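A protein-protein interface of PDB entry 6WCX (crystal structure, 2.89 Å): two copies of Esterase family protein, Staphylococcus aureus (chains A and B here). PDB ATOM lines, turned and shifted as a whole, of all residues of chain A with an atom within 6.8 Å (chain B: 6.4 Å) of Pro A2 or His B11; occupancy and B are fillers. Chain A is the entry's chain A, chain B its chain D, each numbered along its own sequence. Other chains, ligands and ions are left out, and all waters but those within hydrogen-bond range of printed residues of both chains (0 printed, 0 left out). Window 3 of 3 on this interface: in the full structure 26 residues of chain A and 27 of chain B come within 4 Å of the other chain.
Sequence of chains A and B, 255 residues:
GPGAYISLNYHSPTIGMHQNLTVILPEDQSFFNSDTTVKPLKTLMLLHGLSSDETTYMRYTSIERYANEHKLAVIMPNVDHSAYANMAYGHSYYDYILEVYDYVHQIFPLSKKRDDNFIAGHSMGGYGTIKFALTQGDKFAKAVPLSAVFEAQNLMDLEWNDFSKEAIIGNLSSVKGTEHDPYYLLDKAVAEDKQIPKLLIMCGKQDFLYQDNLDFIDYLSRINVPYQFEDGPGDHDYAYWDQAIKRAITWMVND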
ATOM      1  N   GLY A   1      13.096  -2.338  19.190  1.00  0.00           N
ATOM      2  CA  GLY A   1      13.292  -2.675  17.790  1.00  0.00           C
ATOM      3  C   GLY A   1      11.997  -2.818  17.006  1.00  0.00           C
ATOM      4  O   GLY A   1      10.971  -3.183  17.571  1.00  0.00           O
ATOM      5  N   PRO A   2      12.039  -2.554  15.693  1.00  0.00           N
ATOM      6  CA  PRO A   2      10.798  -2.537  14.909  1.00  0.00           C
ATOM      7  C   PRO A   2      10.533  -3.820  14.131  1.00  0.00           C
ATOM      8  O   PRO A   2      11.376  -4.726  14.108  1.00  0.00           O
ATOM      9  CB  PRO A   2      11.032  -1.361  13.962  1.00  0.00           C
ATOM     10  CG  PRO A   2      12.540  -1.435  13.690  1.00  0.00           C
ATOM     11  CD  PRO A   2      13.191  -2.115  14.887  1.00  0.00           C
ATOM     12  N   GLY A   3       9.373  -3.906  13.481  1.00  0.00           N
ATOM     13  CA  GLY A   3       9.016  -5.115  12.777  1.00  0.00           C
ATOM     14  C   GLY A   3       7.952  -4.878  11.733  1.00  0.00           C
ATOM     15  O   GLY A   3       7.555  -3.745  11.468  1.00  0.00           O
ATOM     16  N   ALA A   4       7.478  -5.977  11.158  1.00  0.00           N
ATOM     17  CA  ALA A   4       6.459  -5.972  10.116  1.00  0.00           C
ATOM     18  C   ALA A   4       5.161  -6.579  10.633  1.00  0.00           C
ATOM     19  O   ALA A   4       5.183  -7.628  11.281  1.00  0.00           O
ATOM     20  CB  ALA A   4       6.943  -6.745   8.886  1.00  0.00           C
ATOM     21  N   LEU A  25       6.189 -10.137  12.151  1.00  0.00           N
ATOM     22  CA  LEU A  25       7.535 -10.480  11.699  1.00  0.00           C
ATOM     23  C   LEU A  25       8.474  -9.373  12.143  1.00  0.00           C
ATOM     24  O   LEU A  25       8.560  -8.332  11.465  1.00  0.00           O
ATOM     25  CB  LEU A  25       7.586 -10.655  10.190  1.00  0.00           C
ATOM     26  CG  LEU A  25       8.646 -11.628   9.690  1.00  0.00           C
ATOM     27  CD1 LEU A  25       8.208 -13.056   9.923  1.00  0.00           C
ATOM     28  CD2 LEU A  25       8.929 -11.397   8.213  1.00  0.00           C
ATOM     29  N   PRO A  26       9.186  -9.556  13.262  1.00  0.00           N
ATOM     30  CA  PRO A  26      10.131  -8.534  13.719  1.00  0.00           C
ATOM     31  C   PRO A  26      11.289  -8.396  12.757  1.00  0.00           C
ATOM     32  O   PRO A  26      11.754  -9.371  12.162  1.00  0.00           O
ATOM     33  CB  PRO A  26      10.618  -9.075  15.066  1.00  0.00           C
ATOM     34  CG  PRO A  26       9.621 -10.063  15.462  1.00  0.00           C
ATOM     35  CD  PRO A  26       9.136 -10.685  14.195  1.00  0.00           C
ATOM     36  N   GLU A  27      11.771  -7.169  12.619  1.00  0.00           N
ATOM     37  CA  GLU A  27      12.796  -6.902  11.629  1.00  0.00           C
ATOM     38  C   GLU A  27      14.154  -7.278  12.182  1.00  0.00           C
ATOM     39  O   GLU A  27      14.499  -6.937  13.317  1.00  0.00           O
ATOM     40  CB  GLU A  27      12.801  -5.433  11.215  1.00  0.00           C
ATOM     41  CG  GLU A  27      11.748  -5.070  10.184  1.00  0.00           C
ATOM     42  CD  GLU A  27      11.559  -3.573  10.090  1.00  0.00           C
ATOM     43  OE1 GLU A  27      12.570  -2.848   9.909  1.00  0.00           O
ATOM     44  OE2 GLU A  27      10.398  -3.116  10.216  1.00  0.00           O
ATOM     45  N   ASP A  28      14.907  -8.012  11.386  1.00  0.00           N
ATOM     46  CA  ASP A  28      16.304  -8.277  11.642  1.00  0.00           C
ATOM     47  C   ASP A  28      17.093  -7.456  10.632  1.00  0.00           C
ATOM     48  O   ASP A  28      16.549  -7.019   9.614  1.00  0.00           O
ATOM     49  CB  ASP A  28      16.593  -9.773  11.509  1.00  0.00           C
ATOM     50  CG  ASP A  28      17.898 -10.182  12.158  1.00  0.00           C
ATOM     51  OD1 ASP A  28      17.888 -10.537  13.361  1.00  0.00           O
ATOM     52  OD2 ASP A  28      18.937 -10.131  11.462  1.00  0.00           O
ATOM     53  N   PHE A  32      17.490  -6.575   5.137  1.00  0.00           N
ATOM     54  CA  PHE A  32      17.694  -5.433   4.258  1.00  0.00           C
ATOM     55  C   PHE A  32      19.028  -5.477   3.537  1.00  0.00           C
ATOM     56  O   PHE A  32      19.337  -4.549   2.781  1.00  0.00           O
ATOM     57  CB  PHE A  32      17.603  -4.125   5.050  1.00  0.00           C
ATOM     58  CG  PHE A  32      16.257  -3.870   5.657  1.00  0.00           C
ATOM     59  CD1 PHE A  32      15.239  -3.298   4.903  1.00  0.00           C
ATOM     60  CD2 PHE A  32      16.007  -4.208   6.987  1.00  0.00           C
ATOM     61  CE1 PHE A  32      13.995  -3.059   5.464  1.00  0.00           C
ATOM     62  CE2 PHE A  32      14.763  -3.978   7.561  1.00  0.00           C
ATOM     63  CZ  PHE A  32      13.754  -3.405   6.800  1.00  0.00           C
ATOM     64  N   GLU A  64       2.615  -7.208  19.379  1.00  0.00           N
ATOM     65  CA  GLU A  64       3.699  -6.883  18.451  1.00  0.00           C
ATOM     66  C   GLU A  64       4.788  -6.058  19.123  1.00  0.00           C
ATOM     67  O   GLU A  64       5.970  -6.236  18.811  1.00  0.00           O
ATOM     68  CB  GLU A  64       3.165  -6.144  17.222  1.00  0.00           C
ATOM     69  CG  GLU A  64       4.219  -5.923  16.140  1.00  0.00           C
ATOM     70  CD  GLU A  64       3.711  -5.098  14.984  1.00  0.00           C
ATOM     71  OE1 GLU A  64       2.502  -4.798  14.958  1.00  0.00           O
ATOM     72  OE2 GLU A  64       4.517  -4.757  14.087  1.00  0.00           O
ATOM     73  N   ASN A  68       8.443  -7.786  19.329  1.00  0.00           N
ATOM     74  CA  ASN A  68       9.567  -7.116  18.686  1.00  0.00           C
ATOM     75  C   ASN A  68      10.738  -6.907  19.649  1.00  0.00           C
ATOM     76  O   ASN A  68      11.889  -6.901  19.200  1.00  0.00           O
ATOM     77  CB  ASN A  68       9.116  -5.787  18.070  1.00  0.00           C
ATOM     78  CG  ASN A  68       8.271  -5.970  16.803  1.00  0.00           C
ATOM     79  OD1 ASN A  68       8.013  -7.095  16.366  1.00  0.00           O
ATOM     80  ND2 ASN A  68       7.832  -4.856  16.216  1.00  0.00           N
ATOM     81  N   ASN B   9       3.072  -3.997   6.644  1.00  0.00           N
ATOM     82  CA  ASN B   9       3.411  -2.675   7.154  1.00  0.00           C
ATOM     83  C   ASN B   9       4.619  -2.820   8.061  1.00  0.00           C
ATOM     84  O   ASN B   9       4.514  -3.429   9.129  1.00  0.00           O
ATOM     85  CB  ASN B   9       2.250  -2.046   7.918  1.00  0.00           C
ATOM     86  CG  ASN B   9       2.415  -0.548   8.099  1.00  0.00           C
ATOM     87  OD1 ASN B   9       3.474  -0.062   8.506  1.00  0.00           O
ATOM     88  ND2 ASN B   9       1.351   0.199   7.825  1.00  0.00           N
ATOM     89  N   TYR B  10       5.745  -2.234   7.669  1.00  0.00           N
ATOM     90  CA  TYR B  10       6.953  -2.281   8.480  1.00  0.00           C
ATOM     91  C   TYR B  10       7.569  -0.893   8.581  1.00  0.00           C
ATOM     92  O   TYR B  10       7.276  -0.001   7.779  1.00  0.00           O
ATOM     93  CB  TYR B  10       7.983  -3.277   7.919  1.00  0.00           C
ATOM     94  CG  TYR B  10       8.626  -2.862   6.619  1.00  0.00           C
ATOM     95  CD1 TYR B  10       7.969  -3.050   5.406  1.00  0.00           C
ATOM     96  CD2 TYR B  10       9.898  -2.285   6.598  1.00  0.00           C
ATOM     97  CE1 TYR B  10       8.558  -2.668   4.202  1.00  0.00           C
ATOM     98  CE2 TYR B  10      10.493  -1.902   5.405  1.00  0.00           C
ATOM     99  CZ  TYR B  10       9.820  -2.097   4.211  1.00  0.00           C
ATOM    100  OH  TYR B  10      10.410  -1.721   3.023  1.00  0.00           O
ATOM    101  N   HIS B  11       8.407  -0.711   9.606  1.00  0.00           N
ATOM    102  CA  HIS B  11       9.182   0.519   9.754  1.00  0.00           C
ATOM    103  C   HIS B  11      10.350   0.500   8.774  1.00  0.00           C
ATOM    104  O   HIS B  11      11.251  -0.340   8.882  1.00  0.00           O
ATOM    105  CB  HIS B  11       9.689   0.681  11.188  1.00  0.00           C
ATOM    106  CG  HIS B  11      10.278   2.030  11.472  1.00  0.00           C
ATOM    107  ND1 HIS B  11      11.475   2.455  10.931  1.00  0.00           N
ATOM    108  CD2 HIS B  11       9.835   3.047  12.249  1.00  0.00           C
ATOM    109  CE1 HIS B  11      11.737   3.681  11.352  1.00  0.00           C
ATOM    110  NE2 HIS B  11      10.758   4.063  12.153  1.00  0.00           N
ATOM    111  N   SER B  12      10.330   1.432   7.829  1.00  0.00           N
ATOM    112  CA  SER B  12      11.359   1.530   6.798  1.00  0.00           C
ATOM    113  C   SER B  12      12.574   2.303   7.297  1.00  0.00           C
ATOM    114  O   SER B  12      12.446   3.493   7.612  1.00  0.00           O
ATOM    115  CB  SER B  12      10.801   2.220   5.579  1.00  0.00           C
ATOM    116  OG  SER B  12      11.490   1.818   4.422  1.00  0.00           O
ATOM    117  N   PRO B  13      13.761   1.690   7.359  1.00  0.00           N
ATOM    118  CA  PRO B  13      14.958   2.481   7.667  1.00  0.00           C
ATOM    119  C   PRO B  13      15.333   3.467   6.576  1.00  0.00           C
ATOM    120  O   PRO B  13      16.093   4.406   6.847  1.00  0.00           O
ATOM    121  CB  PRO B  13      16.050   1.414   7.848  1.00  0.00           C
ATOM    122  CG  PRO B  13      15.525   0.184   7.207  1.00  0.00           C
ATOM    123  CD  PRO B  13      14.047   0.247   7.387  1.00  0.00           C
ATOM    124  N   THR B  14      14.811   3.302   5.361  1.00  0.00           N
ATOM    125  CA  THR B  14      15.140   4.233   4.292  1.00  0.00           C
ATOM    126  C   THR B  14      14.308   5.505   4.396  1.00  0.00           C
ATOM    127  O   THR B  14      14.861   6.609   4.482  1.00  0.00           O
ATOM    128  CB  THR B  14      14.967   3.561   2.929  1.00  0.00           C
ATOM    129  OG1 THR B  14      15.873   2.459   2.840  1.00  0.00           O
ATOM    130  CG2 THR B  14      15.286   4.536   1.809  1.00  0.00           C
ATOM    131  N   GLY B  16      12.205   6.280   6.867  1.00  0.00           N
ATOM    132  CA  GLY B  16      12.111   6.732   8.242  1.00  0.00           C
ATOM    133  C   GLY B  16      10.722   6.745   8.828  1.00  0.00           C
ATOM    134  O   GLY B  16      10.438   7.556   9.722  1.00  0.00           O
ATOM    135  N   MET B  17       9.861   5.838   8.383  1.00  0.00           N
ATOM    136  CA  MET B  17       8.504   5.764   8.900  1.00  0.00           C
ATOM    137  C   MET B  17       7.929   4.392   8.578  1.00  0.00           C
ATOM    138  O   MET B  17       8.477   3.634   7.771  1.00  0.00           O
ATOM    139  CB  MET B  17       7.623   6.863   8.308  1.00  0.00           C
ATOM    140  CG  MET B  17       7.444   6.674   6.843  1.00  0.00           C
ATOM    141  SD  MET B  17       6.479   7.949   6.049  1.00  0.00           S
ATOM    142  CE  MET B  17       7.039   7.682   4.373  1.00  0.00           C
ATOM    143  N   HIS B  18       6.814   4.079   9.236  1.00  0.00           N
ATOM    144  CA  HIS B  18       6.013   2.927   8.847  1.00  0.00           C
ATOM    145  C   HIS B  18       5.389   3.167   7.481  1.00  0.00           C
ATOM    146  O   HIS B  18       4.967   4.284   7.159  1.00  0.00           O
ATOM    147  CB  HIS B  18       4.915   2.662   9.870  1.00  0.00           C
ATOM    148  CG  HIS B  18       5.411   2.071  11.145  1.00  0.00           C
ATOM    149  ND1 HIS B  18       6.158   2.788  12.054  1.00  0.00           N
ATOM    150  CD2 HIS B  18       5.266   0.831  11.666  1.00  0.00           C
ATOM    151  CE1 HIS B  18       6.450   2.014  13.084  1.00  0.00           C
ATOM    152  NE2 HIS B  18       5.925   0.820  12.871  1.00  0.00           N
ATOM    153  N   GLN B  19       5.339   2.116   6.671  1.00  0.00           N
ATOM    154  CA  GLN B  19       4.800   2.255   5.329  1.00  0.00           C
ATOM    155  C   GLN B  19       4.102   0.968   4.929  1.00  0.00           C
ATOM    156  O   GLN B  19       4.559  -0.125   5.265  1.00  0.00           O
ATOM    157  CB  GLN B  19       5.902   2.601   4.326  1.00  0.00           C
ATOM    158  CG  GLN B  19       5.395   3.089   2.979  1.00  0.00           C
ATOM    159  CD  GLN B  19       5.161   4.591   2.922  1.00  0.00           C
ATOM    160  OE1 GLN B  19       4.851   5.229   3.930  1.00  0.00           O
ATOM    161  NE2 GLN B  19       5.294   5.160   1.725  1.00  0.00           N
ATOM    162  N   GLU B  99      15.064  -0.713  -1.458  1.00  0.00           N
ATOM    163  CA  GLU B  99      14.845  -1.354  -0.168  1.00  0.00           C
ATOM    164  C   GLU B  99      13.697  -2.363  -0.222  1.00  0.00           C
ATOM    165  O   GLU B  99      13.805  -3.459   0.344  1.00  0.00           O
ATOM    166  CB  GLU B  99      14.575  -0.301   0.897  1.00  0.00           C
ATOM    167  CG  GLU B  99      14.519  -0.884   2.283  1.00  0.00           C
ATOM    168  CD  GLU B  99      13.649  -0.076   3.198  1.00  0.00           C
ATOM    169  OE1 GLU B  99      14.190   0.426   4.195  1.00  0.00           O
ATOM    170  OE2 GLU B  99      12.437   0.069   2.923  1.00  0.00           O
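Pro A2 touches one residue of chain B.
Of the printed residues of chain B, Ala A4 touches Asn B9 and Tyr B10.
Of the printed residues of chain B, Glu A27 touches Tyr B10 and His B11.
Printed residues of chain B within 4 Å of Phe A32: Tyr B10, Pro B13 and Glu B99.
Of the printed residues of chain A, Asn B9 touches Gly A3 (3.8 Å) and Ala A4 (3.4 Å).
Printed residues of chain A within 4 Å of Tyr B10: Gly A3, Ala A4, Glu A27 and Phe A32.
Of chain A, only Pro A2 (3.7 Å), Gly A3 (3.7 Å) and Glu A27 (3.0 Å) come within 4 Å of His B11.
The nearest residue of chain A that does not touch His B11 is Phe A32 (4.5 Å).
No position is printed for both chains.
Of the 11 printed residues of chain A, 5 touch a printed residue of chain B.
Hydrophobic or aromatic side chains of chain A that line the printed part of chain B: Pro A2, Ala A4 and Phe A32.
The side-chain carboxylate (OE2) of Glu A27 sits at hydrogen-bond distance from the backbone NH (N) of His B11.
The side-chain carboxylate of Glu B99 is in hydrogen-bond range of the side-chain hydroxyl of Thr B14 (3.0 Å).
N of Gly A3 lies close to ND2 of Asn A68, 3.3 Å away.
The backbone carbonyl oxygen of Tyr B10 sits at hydrogen-bond distance from the backbone NH of Gln B19.
The side-chain hydroxyl (OH) of Tyr B10 sits at hydrogen-bond distance from the side-chain carboxylate (OE2) of Glu B99, at 2.7 Å.
O of Leu A25 is in hydrogen-bond range of N of Ala A4 (2.6 Å).
OE2 of Glu B99 is in hydrogen-bond range of OG of Ser B12 (2.5 Å).
CB of Pro A2 touches CB of His B11, at 3.7 Å.
O of Gly A3 touches O of Asn B9 (3.8 Å).
Tyr B10 touches Gly A3.
His B11 touches Gly A3.
Asn B9 touches Ala A4 (O to CA, 3.4 Å).
Ala A4 touches Tyr B10.
OE2 of Glu A27 touches CB of Tyr B10, at 3.3 Å.
CE1 of Phe A32 touches CE2 of Tyr B10 (3.7 Å).
Pro B13 touches Phe A32 (CD to CZ, 3.7 Å).
CD1 of Phe A32 touches CG of Glu B99, 3.6 Å away.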
